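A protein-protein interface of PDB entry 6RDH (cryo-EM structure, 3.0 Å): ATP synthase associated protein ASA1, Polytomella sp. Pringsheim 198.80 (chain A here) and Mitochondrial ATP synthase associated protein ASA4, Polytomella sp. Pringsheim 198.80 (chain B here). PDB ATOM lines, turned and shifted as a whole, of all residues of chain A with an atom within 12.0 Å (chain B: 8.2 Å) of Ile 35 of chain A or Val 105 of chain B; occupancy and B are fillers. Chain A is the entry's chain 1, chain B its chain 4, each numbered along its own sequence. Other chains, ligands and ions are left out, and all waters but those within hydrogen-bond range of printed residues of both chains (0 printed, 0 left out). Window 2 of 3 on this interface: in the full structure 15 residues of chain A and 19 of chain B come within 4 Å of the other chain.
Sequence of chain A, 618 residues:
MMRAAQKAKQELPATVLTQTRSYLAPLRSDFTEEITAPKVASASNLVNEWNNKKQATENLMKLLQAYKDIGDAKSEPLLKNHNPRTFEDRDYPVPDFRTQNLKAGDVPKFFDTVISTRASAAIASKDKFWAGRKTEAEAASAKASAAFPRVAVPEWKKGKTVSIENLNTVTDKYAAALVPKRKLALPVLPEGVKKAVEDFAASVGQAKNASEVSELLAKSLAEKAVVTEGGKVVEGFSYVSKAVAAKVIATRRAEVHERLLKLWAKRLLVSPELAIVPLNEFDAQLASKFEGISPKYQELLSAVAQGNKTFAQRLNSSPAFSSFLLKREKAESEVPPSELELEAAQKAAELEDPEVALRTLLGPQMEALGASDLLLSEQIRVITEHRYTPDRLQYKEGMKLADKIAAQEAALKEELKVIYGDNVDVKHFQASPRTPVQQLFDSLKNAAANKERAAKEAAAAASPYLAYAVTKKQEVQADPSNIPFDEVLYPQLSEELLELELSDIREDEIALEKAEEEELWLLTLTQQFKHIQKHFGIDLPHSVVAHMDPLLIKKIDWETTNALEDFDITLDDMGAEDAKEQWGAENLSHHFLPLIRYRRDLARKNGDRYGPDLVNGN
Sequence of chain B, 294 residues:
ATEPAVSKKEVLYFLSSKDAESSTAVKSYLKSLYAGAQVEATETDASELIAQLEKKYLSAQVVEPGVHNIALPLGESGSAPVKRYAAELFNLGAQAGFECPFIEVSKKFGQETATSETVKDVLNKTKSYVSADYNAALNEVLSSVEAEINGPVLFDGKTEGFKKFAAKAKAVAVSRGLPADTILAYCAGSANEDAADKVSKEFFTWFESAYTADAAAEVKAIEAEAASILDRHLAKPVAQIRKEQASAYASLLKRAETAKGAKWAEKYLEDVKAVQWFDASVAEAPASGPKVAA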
ATOM      1  N   PHE A  31     -22.918  30.937  29.544  1.00  0.00           N
ATOM      2  CA  PHE A  31     -23.477  30.036  28.558  1.00  0.00           C
ATOM      3  C   PHE A  31     -24.410  29.047  29.234  1.00  0.00           C
ATOM      4  O   PHE A  31     -24.332  28.813  30.440  1.00  0.00           O
ATOM      5  CB  PHE A  31     -22.369  29.295  27.814  1.00  0.00           C
ATOM      6  CG  PHE A  31     -21.579  30.163  26.885  1.00  0.00           C
ATOM      7  CD1 PHE A  31     -21.849  30.169  25.537  1.00  0.00           C
ATOM      8  CD2 PHE A  31     -20.562  30.969  27.360  1.00  0.00           C
ATOM      9  CE1 PHE A  31     -21.130  30.965  24.686  1.00  0.00           C
ATOM     10  CE2 PHE A  31     -19.842  31.768  26.507  1.00  0.00           C
ATOM     11  CZ  PHE A  31     -20.124  31.764  25.175  1.00  0.00           C
ATOM     12  N   THR A  32     -25.305  28.472  28.440  1.00  0.00           N
ATOM     13  CA  THR A  32     -26.258  27.482  28.922  1.00  0.00           C
ATOM     14  C   THR A  32     -25.811  26.115  28.430  1.00  0.00           C
ATOM     15  O   THR A  32     -26.077  25.744  27.285  1.00  0.00           O
ATOM     16  CB  THR A  32     -27.667  27.804  28.443  1.00  0.00           C
ATOM     17  OG1 THR A  32     -27.959  29.171  28.733  1.00  0.00           O
ATOM     18  CG2 THR A  32     -28.666  26.945  29.155  1.00  0.00           C
ATOM     19  N   GLU A  33     -25.139  25.362  29.297  1.00  0.00           N
ATOM     20  CA  GLU A  33     -24.571  24.086  28.900  1.00  0.00           C
ATOM     21  C   GLU A  33     -25.582  22.953  28.872  1.00  0.00           C
ATOM     22  O   GLU A  33     -25.291  21.901  28.298  1.00  0.00           O
ATOM     23  CB  GLU A  33     -23.419  23.708  29.830  1.00  0.00           C
ATOM     24  CG  GLU A  33     -22.176  24.548  29.644  1.00  0.00           C
ATOM     25  CD  GLU A  33     -22.068  25.654  30.663  1.00  0.00           C
ATOM     26  OE1 GLU A  33     -22.988  25.780  31.497  1.00  0.00           O
ATOM     27  OE2 GLU A  33     -21.063  26.394  30.636  1.00  0.00           O
ATOM     28  N   GLU A  34     -26.746  23.128  29.477  1.00  0.00           N
ATOM     29  CA  GLU A  34     -27.769  22.097  29.459  1.00  0.00           C
ATOM     30  C   GLU A  34     -28.860  22.455  28.464  1.00  0.00           C
ATOM     31  O   GLU A  34     -28.958  23.587  27.997  1.00  0.00           O
ATOM     32  CB  GLU A  34     -28.372  21.908  30.849  1.00  0.00           C
ATOM     33  CG  GLU A  34     -29.067  23.140  31.409  1.00  0.00           C
ATOM     34  CD  GLU A  34     -28.142  24.050  32.201  1.00  0.00           C
ATOM     35  OE1 GLU A  34     -26.916  23.811  32.200  1.00  0.00           O
ATOM     36  OE2 GLU A  34     -28.643  25.012  32.820  1.00  0.00           O
ATOM     37  N   ILE A  35     -29.681  21.473  28.131  1.00  0.00           N
ATOM     38  CA  ILE A  35     -30.877  21.702  27.336  1.00  0.00           C
ATOM     39  C   ILE A  35     -32.063  21.329  28.204  1.00  0.00           C
ATOM     40  O   ILE A  35     -32.282  20.148  28.498  1.00  0.00           O
ATOM     41  CB  ILE A  35     -30.877  20.915  26.026  1.00  0.00           C
ATOM     42  CG1 ILE A  35     -29.743  21.389  25.135  1.00  0.00           C
ATOM     43  CG2 ILE A  35     -32.190  21.098  25.312  1.00  0.00           C
ATOM     44  CD1 ILE A  35     -29.633  20.622  23.867  1.00  0.00           C
ATOM     45  N   THR A  36     -32.825  22.334  28.619  1.00  0.00           N
ATOM     46  CA  THR A  36     -33.895  22.172  29.584  1.00  0.00           C
ATOM     47  C   THR A  36     -35.152  22.818  29.009  1.00  0.00           C
ATOM     48  O   THR A  36     -35.075  23.769  28.231  1.00  0.00           O
ATOM     49  CB  THR A  36     -33.473  22.810  30.925  1.00  0.00           C
ATOM     50  OG1 THR A  36     -32.272  22.182  31.379  1.00  0.00           O
ATOM     51  CG2 THR A  36     -34.497  22.598  32.022  1.00  0.00           C
ATOM     52  N   ALA A  37     -36.309  22.244  29.341  1.00  0.00           N
ATOM     53  CA  ALA A  37     -37.586  22.893  29.108  1.00  0.00           C
ATOM     54  C   ALA A  37     -37.625  24.226  29.856  1.00  0.00           C
ATOM     55  O   ALA A  37     -37.086  24.342  30.959  1.00  0.00           O
ATOM     56  CB  ALA A  37     -38.720  21.983  29.570  1.00  0.00           C
ATOM     57  N   PRO A  38     -38.266  25.255  29.289  1.00  0.00           N
ATOM     58  CA  PRO A  38     -37.912  26.620  29.680  1.00  0.00           C
ATOM     59  C   PRO A  38     -38.556  27.133  30.961  1.00  0.00           C
ATOM     60  O   PRO A  38     -38.530  28.348  31.188  1.00  0.00           O
ATOM     61  CB  PRO A  38     -38.367  27.448  28.472  1.00  0.00           C
ATOM     62  CG  PRO A  38     -38.876  26.481  27.467  1.00  0.00           C
ATOM     63  CD  PRO A  38     -39.265  25.279  28.215  1.00  0.00           C
ATOM     64  N   LYS A  39     -39.095  26.238  31.797  1.00  0.00           N
ATOM     65  CA  LYS A  39     -39.569  26.524  33.159  1.00  0.00           C
ATOM     66  C   LYS A  39     -40.678  27.583  33.166  1.00  0.00           C
ATOM     67  O   LYS A  39     -40.483  28.735  33.555  1.00  0.00           O
ATOM     68  CB  LYS A  39     -38.395  26.931  34.060  1.00  0.00           C
ATOM     69  CG  LYS A  39     -38.693  26.924  35.544  1.00  0.00           C
ATOM     70  CD  LYS A  39     -37.500  27.421  36.332  1.00  0.00           C
ATOM     71  CE  LYS A  39     -36.351  26.440  36.247  1.00  0.00           C
ATOM     72  NZ  LYS A  39     -36.689  25.142  36.885  1.00  0.00           N
ATOM     73  N   GLU B  99     -24.153  24.573  12.715  1.00  0.00           N
ATOM     74  CA  GLU B  99     -24.760  23.716  11.714  1.00  0.00           C
ATOM     75  C   GLU B  99     -26.271  23.736  11.918  1.00  0.00           C
ATOM     76  O   GLU B  99     -26.806  24.650  12.545  1.00  0.00           O
ATOM     77  CB  GLU B  99     -24.175  22.314  11.814  1.00  0.00           C
ATOM     78  CG  GLU B  99     -23.029  22.046  10.896  1.00  0.00           C
ATOM     79  CD  GLU B  99     -22.619  20.600  10.935  1.00  0.00           C
ATOM     80  OE1 GLU B  99     -22.206  20.123  12.011  1.00  0.00           O
ATOM     81  OE2 GLU B  99     -22.729  19.927   9.893  1.00  0.00           O
ATOM     82  N   CYS B 100     -26.979  22.766  11.350  1.00  0.00           N
ATOM     83  CA  CYS B 100     -28.339  22.482  11.779  1.00  0.00           C
ATOM     84  C   CYS B 100     -28.341  22.101  13.259  1.00  0.00           C
ATOM     85  O   CYS B 100     -27.357  21.556  13.764  1.00  0.00           O
ATOM     86  CB  CYS B 100     -28.919  21.346  10.944  1.00  0.00           C
ATOM     87  SG  CYS B 100     -30.699  21.107  11.020  1.00  0.00           S
ATOM     88  N   PRO B 101     -29.410  22.430  13.987  1.00  0.00           N
ATOM     89  CA  PRO B 101     -29.506  22.018  15.396  1.00  0.00           C
ATOM     90  C   PRO B 101     -29.485  20.521  15.603  1.00  0.00           C
ATOM     91  O   PRO B 101     -28.929  20.056  16.606  1.00  0.00           O
ATOM     92  CB  PRO B 101     -30.846  22.613  15.829  1.00  0.00           C
ATOM     93  CG  PRO B 101     -31.013  23.776  14.993  1.00  0.00           C
ATOM     94  CD  PRO B 101     -30.347  23.515  13.685  1.00  0.00           C
ATOM     95  N   PHE B 102     -30.061  19.761  14.670  1.00  0.00           N
ATOM     96  CA  PHE B 102     -30.014  18.307  14.728  1.00  0.00           C
ATOM     97  C   PHE B 102     -28.582  17.806  14.636  1.00  0.00           C
ATOM     98  O   PHE B 102     -28.137  16.999  15.462  1.00  0.00           O
ATOM     99  CB  PHE B 102     -30.857  17.733  13.595  1.00  0.00           C
ATOM    100  CG  PHE B 102     -31.189  16.293  13.761  1.00  0.00           C
ATOM    101  CD1 PHE B 102     -30.448  15.322  13.122  1.00  0.00           C
ATOM    102  CD2 PHE B 102     -32.250  15.909  14.552  1.00  0.00           C
ATOM    103  CE1 PHE B 102     -30.759  13.995  13.273  1.00  0.00           C
ATOM    104  CE2 PHE B 102     -32.564  14.588  14.703  1.00  0.00           C
ATOM    105  CZ  PHE B 102     -31.816  13.630  14.066  1.00  0.00           C
ATOM    106  N   ILE B 103     -27.835  18.313  13.654  1.00  0.00           N
ATOM    107  CA  ILE B 103     -26.448  17.916  13.463  1.00  0.00           C
ATOM    108  C   ILE B 103     -25.584  18.377  14.623  1.00  0.00           C
ATOM    109  O   ILE B 103     -24.680  17.654  15.056  1.00  0.00           O
ATOM    110  CB  ILE B 103     -25.928  18.462  12.126  1.00  0.00           C
ATOM    111  CG1 ILE B 103     -26.930  18.168  11.019  1.00  0.00           C
ATOM    112  CG2 ILE B 103     -24.631  17.819  11.779  1.00  0.00           C
ATOM    113  CD1 ILE B 103     -26.504  18.672   9.665  1.00  0.00           C
ATOM    114  N   GLU B 104     -25.886  19.538  15.195  1.00  0.00           N
ATOM    115  CA  GLU B 104     -25.044  20.063  16.259  1.00  0.00           C
ATOM    116  C   GLU B 104     -25.262  19.328  17.575  1.00  0.00           C
ATOM    117  O   GLU B 104     -24.295  19.018  18.278  1.00  0.00           O
ATOM    118  CB  GLU B 104     -25.293  21.551  16.435  1.00  0.00           C
ATOM    119  CG  GLU B 104     -24.135  22.251  17.068  1.00  0.00           C
ATOM    120  CD  GLU B 104     -23.274  22.957  16.065  1.00  0.00           C
ATOM    121  OE1 GLU B 104     -23.723  23.117  14.920  1.00  0.00           O
ATOM    122  OE2 GLU B 104     -22.152  23.367  16.418  1.00  0.00           O
ATOM    123  N   VAL B 105     -26.507  19.006  17.925  1.00  0.00           N
ATOM    124  CA  VAL B 105     -26.702  18.254  19.162  1.00  0.00           C
ATOM    125  C   VAL B 105     -26.356  16.778  18.983  1.00  0.00           C
ATOM    126  O   VAL B 105     -25.928  16.133  19.949  1.00  0.00           O
ATOM    127  CB  VAL B 105     -28.125  18.465  19.713  1.00  0.00           C
ATOM    128  CG1 VAL B 105     -29.144  17.749  18.906  1.00  0.00           C
ATOM    129  CG2 VAL B 105     -28.218  18.055  21.171  1.00  0.00           C
ATOM    130  N   SER B 106     -26.438  16.232  17.764  1.00  0.00           N
ATOM    131  CA  SER B 106     -25.933  14.883  17.552  1.00  0.00           C
ATOM    132  C   SER B 106     -24.412  14.853  17.618  1.00  0.00           C
ATOM    133  O   SER B 106     -23.826  13.869  18.076  1.00  0.00           O
ATOM    134  CB  SER B 106     -26.440  14.344  16.224  1.00  0.00           C
ATOM    135  OG  SER B 106     -25.919  15.095  15.154  1.00  0.00           O
ATOM    136  N   LYS B 107     -23.758  15.936  17.193  1.00  0.00           N
ATOM    137  CA  LYS B 107     -22.324  16.081  17.414  1.00  0.00           C
ATOM    138  C   LYS B 107     -21.995  16.192  18.895  1.00  0.00           C
ATOM    139  O   LYS B 107     -20.966  15.676  19.338  1.00  0.00           O
ATOM    140  CB  LYS B 107     -21.809  17.303  16.660  1.00  0.00           C
ATOM    141  CG  LYS B 107     -20.318  17.521  16.751  1.00  0.00           C
ATOM    142  CD  LYS B 107     -19.862  18.640  15.847  1.00  0.00           C
ATOM    143  CE  LYS B 107     -20.368  19.980  16.318  1.00  0.00           C
ATOM    144  NZ  LYS B 107     -19.982  21.062  15.381  1.00  0.00           N
ATOM    145  N   LYS B 108     -22.862  16.841  19.671  1.00  0.00           N
ATOM    146  CA  LYS B 108     -22.673  16.901  21.120  1.00  0.00           C
ATOM    147  C   LYS B 108     -22.791  15.519  21.754  1.00  0.00           C
ATOM    148  O   LYS B 108     -22.029  15.180  22.668  1.00  0.00           O
ATOM    149  CB  LYS B 108     -23.688  17.858  21.740  1.00  0.00           C
ATOM    150  CG  LYS B 108     -23.193  18.552  22.983  1.00  0.00           C
ATOM    151  CD  LYS B 108     -22.109  19.553  22.643  1.00  0.00           C
ATOM    152  CE  LYS B 108     -21.635  20.289  23.877  1.00  0.00           C
ATOM    153  NZ  LYS B 108     -20.598  21.299  23.563  1.00  0.00           N
ATOM    154  N   PHE B 109     -23.730  14.707  21.264  1.00  0.00           N
ATOM    155  CA  PHE B 109     -23.859  13.335  21.748  1.00  0.00           C
ATOM    156  C   PHE B 109     -22.653  12.491  21.362  1.00  0.00           C
ATOM    157  O   PHE B 109     -22.177  11.677  22.158  1.00  0.00           O
ATOM    158  CB  PHE B 109     -25.127  12.695  21.194  1.00  0.00           C
ATOM    159  CG  PHE B 109     -26.382  13.342  21.651  1.00  0.00           C
ATOM    160  CD1 PHE B 109     -26.471  13.886  22.908  1.00  0.00           C
ATOM    161  CD2 PHE B 109     -27.481  13.395  20.822  1.00  0.00           C
ATOM    162  CE1 PHE B 109     -27.626  14.481  23.326  1.00  0.00           C
ATOM    163  CE2 PHE B 109     -28.640  13.986  21.237  1.00  0.00           C
ATOM    164  CZ  PHE B 109     -28.710  14.533  22.491  1.00  0.00           C
ATOM    165  N   GLY B 110     -22.155  12.657  20.138  1.00  0.00           N
ATOM    166  CA  GLY B 110     -21.009  11.877  19.712  1.00  0.00           C
ATOM    167  C   GLY B 110     -19.724  12.296  20.389  1.00  0.00           C
ATOM    168  O   GLY B 110     -18.813  11.482  20.557  1.00  0.00           O
ATOM    169  N   GLN B 111     -19.635  13.559  20.795  1.00  0.00           N
ATOM    170  CA  GLN B 111     -18.465  14.035  21.517  1.00  0.00           C
ATOM    171  C   GLN B 111     -18.512  13.621  22.978  1.00  0.00           C
ATOM    172  O   GLN B 111     -17.472  13.313  23.568  1.00  0.00           O
ATOM    173  CB  GLN B 111     -18.372  15.553  21.381  1.00  0.00           C
ATOM    174  CG  GLN B 111     -17.210  16.198  22.097  1.00  0.00           C
ATOM    175  CD  GLN B 111     -17.160  17.687  21.863  1.00  0.00           C
ATOM    176  OE1 GLN B 111     -17.603  18.174  20.824  1.00  0.00           O
ATOM    177  NE2 GLN B 111     -16.621  18.420  22.826  1.00  0.00           N
ATOM    178  N   GLU B 112     -19.706  13.594  23.575  1.00  0.00           N
ATOM    179  CA  GLU B 112     -19.820  13.226  24.984  1.00  0.00           C
ATOM    180  C   GLU B 112     -19.541  11.745  25.201  1.00  0.00           C
ATOM    181  O   GLU B 112     -18.816  11.370  26.128  1.00  0.00           O
ATOM    182  CB  GLU B 112     -21.207  13.584  25.514  1.00  0.00           C
ATOM    183  CG  GLU B 112     -21.367  15.042  25.868  1.00  0.00           C
ATOM    184  CD  GLU B 112     -20.504  15.455  27.029  1.00  0.00           C
ATOM    185  OE1 GLU B 112     -20.371  14.666  27.982  1.00  0.00           O
ATOM    186  OE2 GLU B 112     -19.948  16.569  26.984  1.00  0.00           O
ATOM    187  N   THR B 126     -25.047  11.844  28.618  1.00  0.00           N
ATOM    188  CA  THR B 126     -25.970  12.742  27.937  1.00  0.00           C
ATOM    189  C   THR B 126     -27.152  13.114  28.805  1.00  0.00           C
ATOM    190  O   THR B 126     -28.259  13.298  28.288  1.00  0.00           O
ATOM    191  CB  THR B 126     -26.470  12.128  26.634  1.00  0.00           C
ATOM    192  OG1 THR B 126     -27.432  11.113  26.932  1.00  0.00           O
ATOM    193  CG2 THR B 126     -25.341  11.544  25.847  1.00  0.00           C
ATOM    194  N   LYS B 127     -26.953  13.183  30.122  1.00  0.00           N
ATOM    195  CA  LYS B 127     -28.032  13.556  31.024  1.00  0.00           C
ATOM    196  C   LYS B 127     -28.425  15.009  30.828  1.00  0.00           C
ATOM    197  O   LYS B 127     -29.611  15.351  30.892  1.00  0.00           O
ATOM    198  CB  LYS B 127     -27.605  13.307  32.468  1.00  0.00           C
ATOM    199  CG  LYS B 127     -28.750  13.319  33.446  1.00  0.00           C
ATOM    200  CD  LYS B 127     -28.304  12.918  34.838  1.00  0.00           C
ATOM    201  CE  LYS B 127     -29.506  12.765  35.761  1.00  0.00           C
ATOM    202  NZ  LYS B 127     -29.123  12.355  37.139  1.00  0.00           N
ATOM    203  N   SER B 128     -27.447  15.868  30.552  1.00  0.00           N
ATOM    204  CA  SER B 128     -27.683  17.299  30.464  1.00  0.00           C
ATOM    205  C   SER B 128     -28.355  17.727  29.173  1.00  0.00           C
ATOM    206  O   SER B 128     -28.847  18.853  29.109  1.00  0.00           O
ATOM    207  CB  SER B 128     -26.366  18.050  30.614  1.00  0.00           C
ATOM    208  OG  SER B 128     -25.829  17.872  31.909  1.00  0.00           O
ATOM    209  N   TYR B 129     -28.402  16.884  28.150  1.00  0.00           N
ATOM    210  CA  TYR B 129     -28.906  17.327  26.863  1.00  0.00           C
ATOM    211  C   TYR B 129     -30.221  16.690  26.455  1.00  0.00           C
ATOM    212  O   TYR B 129     -30.803  17.112  25.456  1.00  0.00           O
ATOM    213  CB  TYR B 129     -27.868  17.072  25.767  1.00  0.00           C
ATOM    214  CG  TYR B 129     -26.516  17.650  26.071  1.00  0.00           C
ATOM    215  CD1 TYR B 129     -26.266  18.999  25.902  1.00  0.00           C
ATOM    216  CD2 TYR B 129     -25.489  16.846  26.523  1.00  0.00           C
ATOM    217  CE1 TYR B 129     -25.033  19.530  26.179  1.00  0.00           C
ATOM    218  CE2 TYR B 129     -24.252  17.367  26.803  1.00  0.00           C
ATOM    219  CZ  TYR B 129     -24.028  18.708  26.631  1.00  0.00           C
ATOM    220  OH  TYR B 129     -22.786  19.226  26.912  1.00  0.00           O
ATOM    221  N   VAL B 130     -30.704  15.694  27.172  1.00  0.00           N
ATOM    222  CA  VAL B 130     -32.011  15.125  26.884  1.00  0.00           C
ATOM    223  C   VAL B 130     -32.953  15.493  28.018  1.00  0.00           C
ATOM    224  O   VAL B 130     -32.523  15.773  29.144  1.00  0.00           O
ATOM    225  CB  VAL B 130     -31.948  13.599  26.672  1.00  0.00           C
ATOM    226  CG1 VAL B 130     -30.951  13.279  25.594  1.00  0.00           C
ATOM    227  CG2 VAL B 130     -31.559  12.893  27.947  1.00  0.00           C
ATOM    228  N   SER B 131     -34.243  15.537  27.703  1.00  0.00           N
ATOM    229  CA  SER B 131     -35.237  15.857  28.713  1.00  0.00           C
ATOM    230  C   SER B 131     -35.323  14.721  29.714  1.00  0.00           C
ATOM    231  O   SER B 131     -35.250  13.550  29.340  1.00  0.00           O
ATOM    232  CB  SER B 131     -36.598  16.094  28.067  1.00  0.00           C
ATOM    233  OG  SER B 131     -36.977  14.996  27.265  1.00  0.00           O
ATOM    234  N   ALA B 132     -35.454  15.069  30.994  1.00  0.00           N
ATOM    235  CA  ALA B 132     -35.443  14.060  32.045  1.00  0.00           C
ATOM    236  C   ALA B 132     -36.656  13.137  31.982  1.00  0.00           C
ATOM    237  O   ALA B 132     -36.568  11.995  32.446  1.00  0.00           O
ATOM    238  CB  ALA B 132     -35.355  14.730  33.414  1.00  0.00           C
ATOM    239  N   PHE B 207     -39.431  17.688  11.869  1.00  0.00           N
ATOM    240  CA  PHE B 207     -38.456  18.673  12.310  1.00  0.00           C
ATOM    241  C   PHE B 207     -39.098  20.033  12.499  1.00  0.00           C
ATOM    242  O   PHE B 207     -38.792  20.735  13.465  1.00  0.00           O
ATOM    243  CB  PHE B 207     -37.320  18.747  11.301  1.00  0.00           C
ATOM    244  CG  PHE B 207     -36.151  19.533  11.770  1.00  0.00           C
ATOM    245  CD1 PHE B 207     -35.506  19.204  12.939  1.00  0.00           C
ATOM    246  CD2 PHE B 207     -35.685  20.597  11.029  1.00  0.00           C
ATOM    247  CE1 PHE B 207     -34.425  19.925  13.364  1.00  0.00           C
ATOM    248  CE2 PHE B 207     -34.606  21.318  11.450  1.00  0.00           C
ATOM    249  CZ  PHE B 207     -33.976  20.980  12.618  1.00  0.00           C
ATOM    250  N   ASP B 214     -40.485  23.735  20.262  1.00  0.00           N
ATOM    251  CA  ASP B 214     -39.475  24.268  21.175  1.00  0.00           C
ATOM    252  C   ASP B 214     -39.532  25.786  21.261  1.00  0.00           C
ATOM    253  O   ASP B 214     -39.410  26.358  22.353  1.00  0.00           O
ATOM    254  CB  ASP B 214     -38.088  23.834  20.732  1.00  0.00           C
ATOM    255  CG  ASP B 214     -37.893  22.357  20.836  1.00  0.00           C
ATOM    256  OD1 ASP B 214     -38.569  21.732  21.673  1.00  0.00           O
ATOM    257  OD2 ASP B 214     -37.053  21.823  20.090  1.00  0.00           O
ATOM    258  N   GLU B 218     -40.445  28.170  24.524  1.00  0.00           N
ATOM    259  CA  GLU B 218     -39.691  29.351  24.953  1.00  0.00           C
ATOM    260  C   GLU B 218     -40.559  30.599  25.014  1.00  0.00           C
ATOM    261  O   GLU B 218     -40.452  31.377  25.970  1.00  0.00           O
ATOM    262  CB  GLU B 218     -38.516  29.605  24.014  1.00  0.00           C
ATOM    263  CG  GLU B 218     -37.446  28.542  24.050  1.00  0.00           C
ATOM    264  CD  GLU B 218     -36.570  28.625  25.281  1.00  0.00           C
ATOM    265  OE1 GLU B 218     -36.310  29.749  25.755  1.00  0.00           O
ATOM    266  OE2 GLU B 218     -36.134  27.565  25.775  1.00  0.00           O
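The backbone NH of Ile 35 of chain A lies within hydrogen-bond range of the backbone carbonyl oxygen of Ser 128 of chain B (2.9 Å).
Glu 33 of chain A touches Tyr 129 of chain B. O of Ser 128 of chain B touches CA of Glu 34 of chain A (3.4 Å). Val 105 of chain B touches Ile 35 of chain A (CG2 to CD1, 3.98 Å). O of Tyr 129 of chain B touches CB of Ile 35 of chain A (3.8 Å). Pro 38 of chain A touches Glu 218 of chain B.
Printed residues of chain B within 4 Å of Glu 33 of chain A: Tyr 129. Of the printed residues of chain B, Ile 35 of chain A touches Val 105 (3.98 Å), Ser 128 (2.9 Å) and Tyr 129 (3.8 Å). Of the printed residues of chain B, Pro 38 of chain A touches Glu 218. Lys 39 of chain A touches none of the printed residues of chain B. No residue of chain A comes within 4 Å of Pro 101 of chain B. No residue of chain A comes within 4 Å of Phe 102 of chain B. No residue of chain A comes within 4 Å of Ser 106 of chain B. No residue of chain A comes within 4 Å of Lys 107 of chain B. Glu 112 of chain B touches none of the printed residues of chain A. Of chain A, only Glu 34 (3.4 Å) and Ile 35 (2.9 Å) come within 4 Å of Ser 128 of chain B. Printed residues of chain A within 4 Å of Tyr 129 of chain B: Glu 33 (3.2 Å) and Ile 35 (3.8 Å). No residue of chain A comes within 4 Å of Ser 131 of chain B. Printed residues of chain A within 4 Å of Glu 218 of chain B: Pro 38. The nearest printed residue of chain A that does not touch Val 105 of chain B is Glu 34 of chain A (8.5 Å).
Hydrophobic or aromatic side chains of chain B that line the printed part of chain A: Val 105 and Tyr 129. Hydrophobic or aromatic side chains of chain A within 4 Å of the printed part of chain B: Ile 35 and Pro 38.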
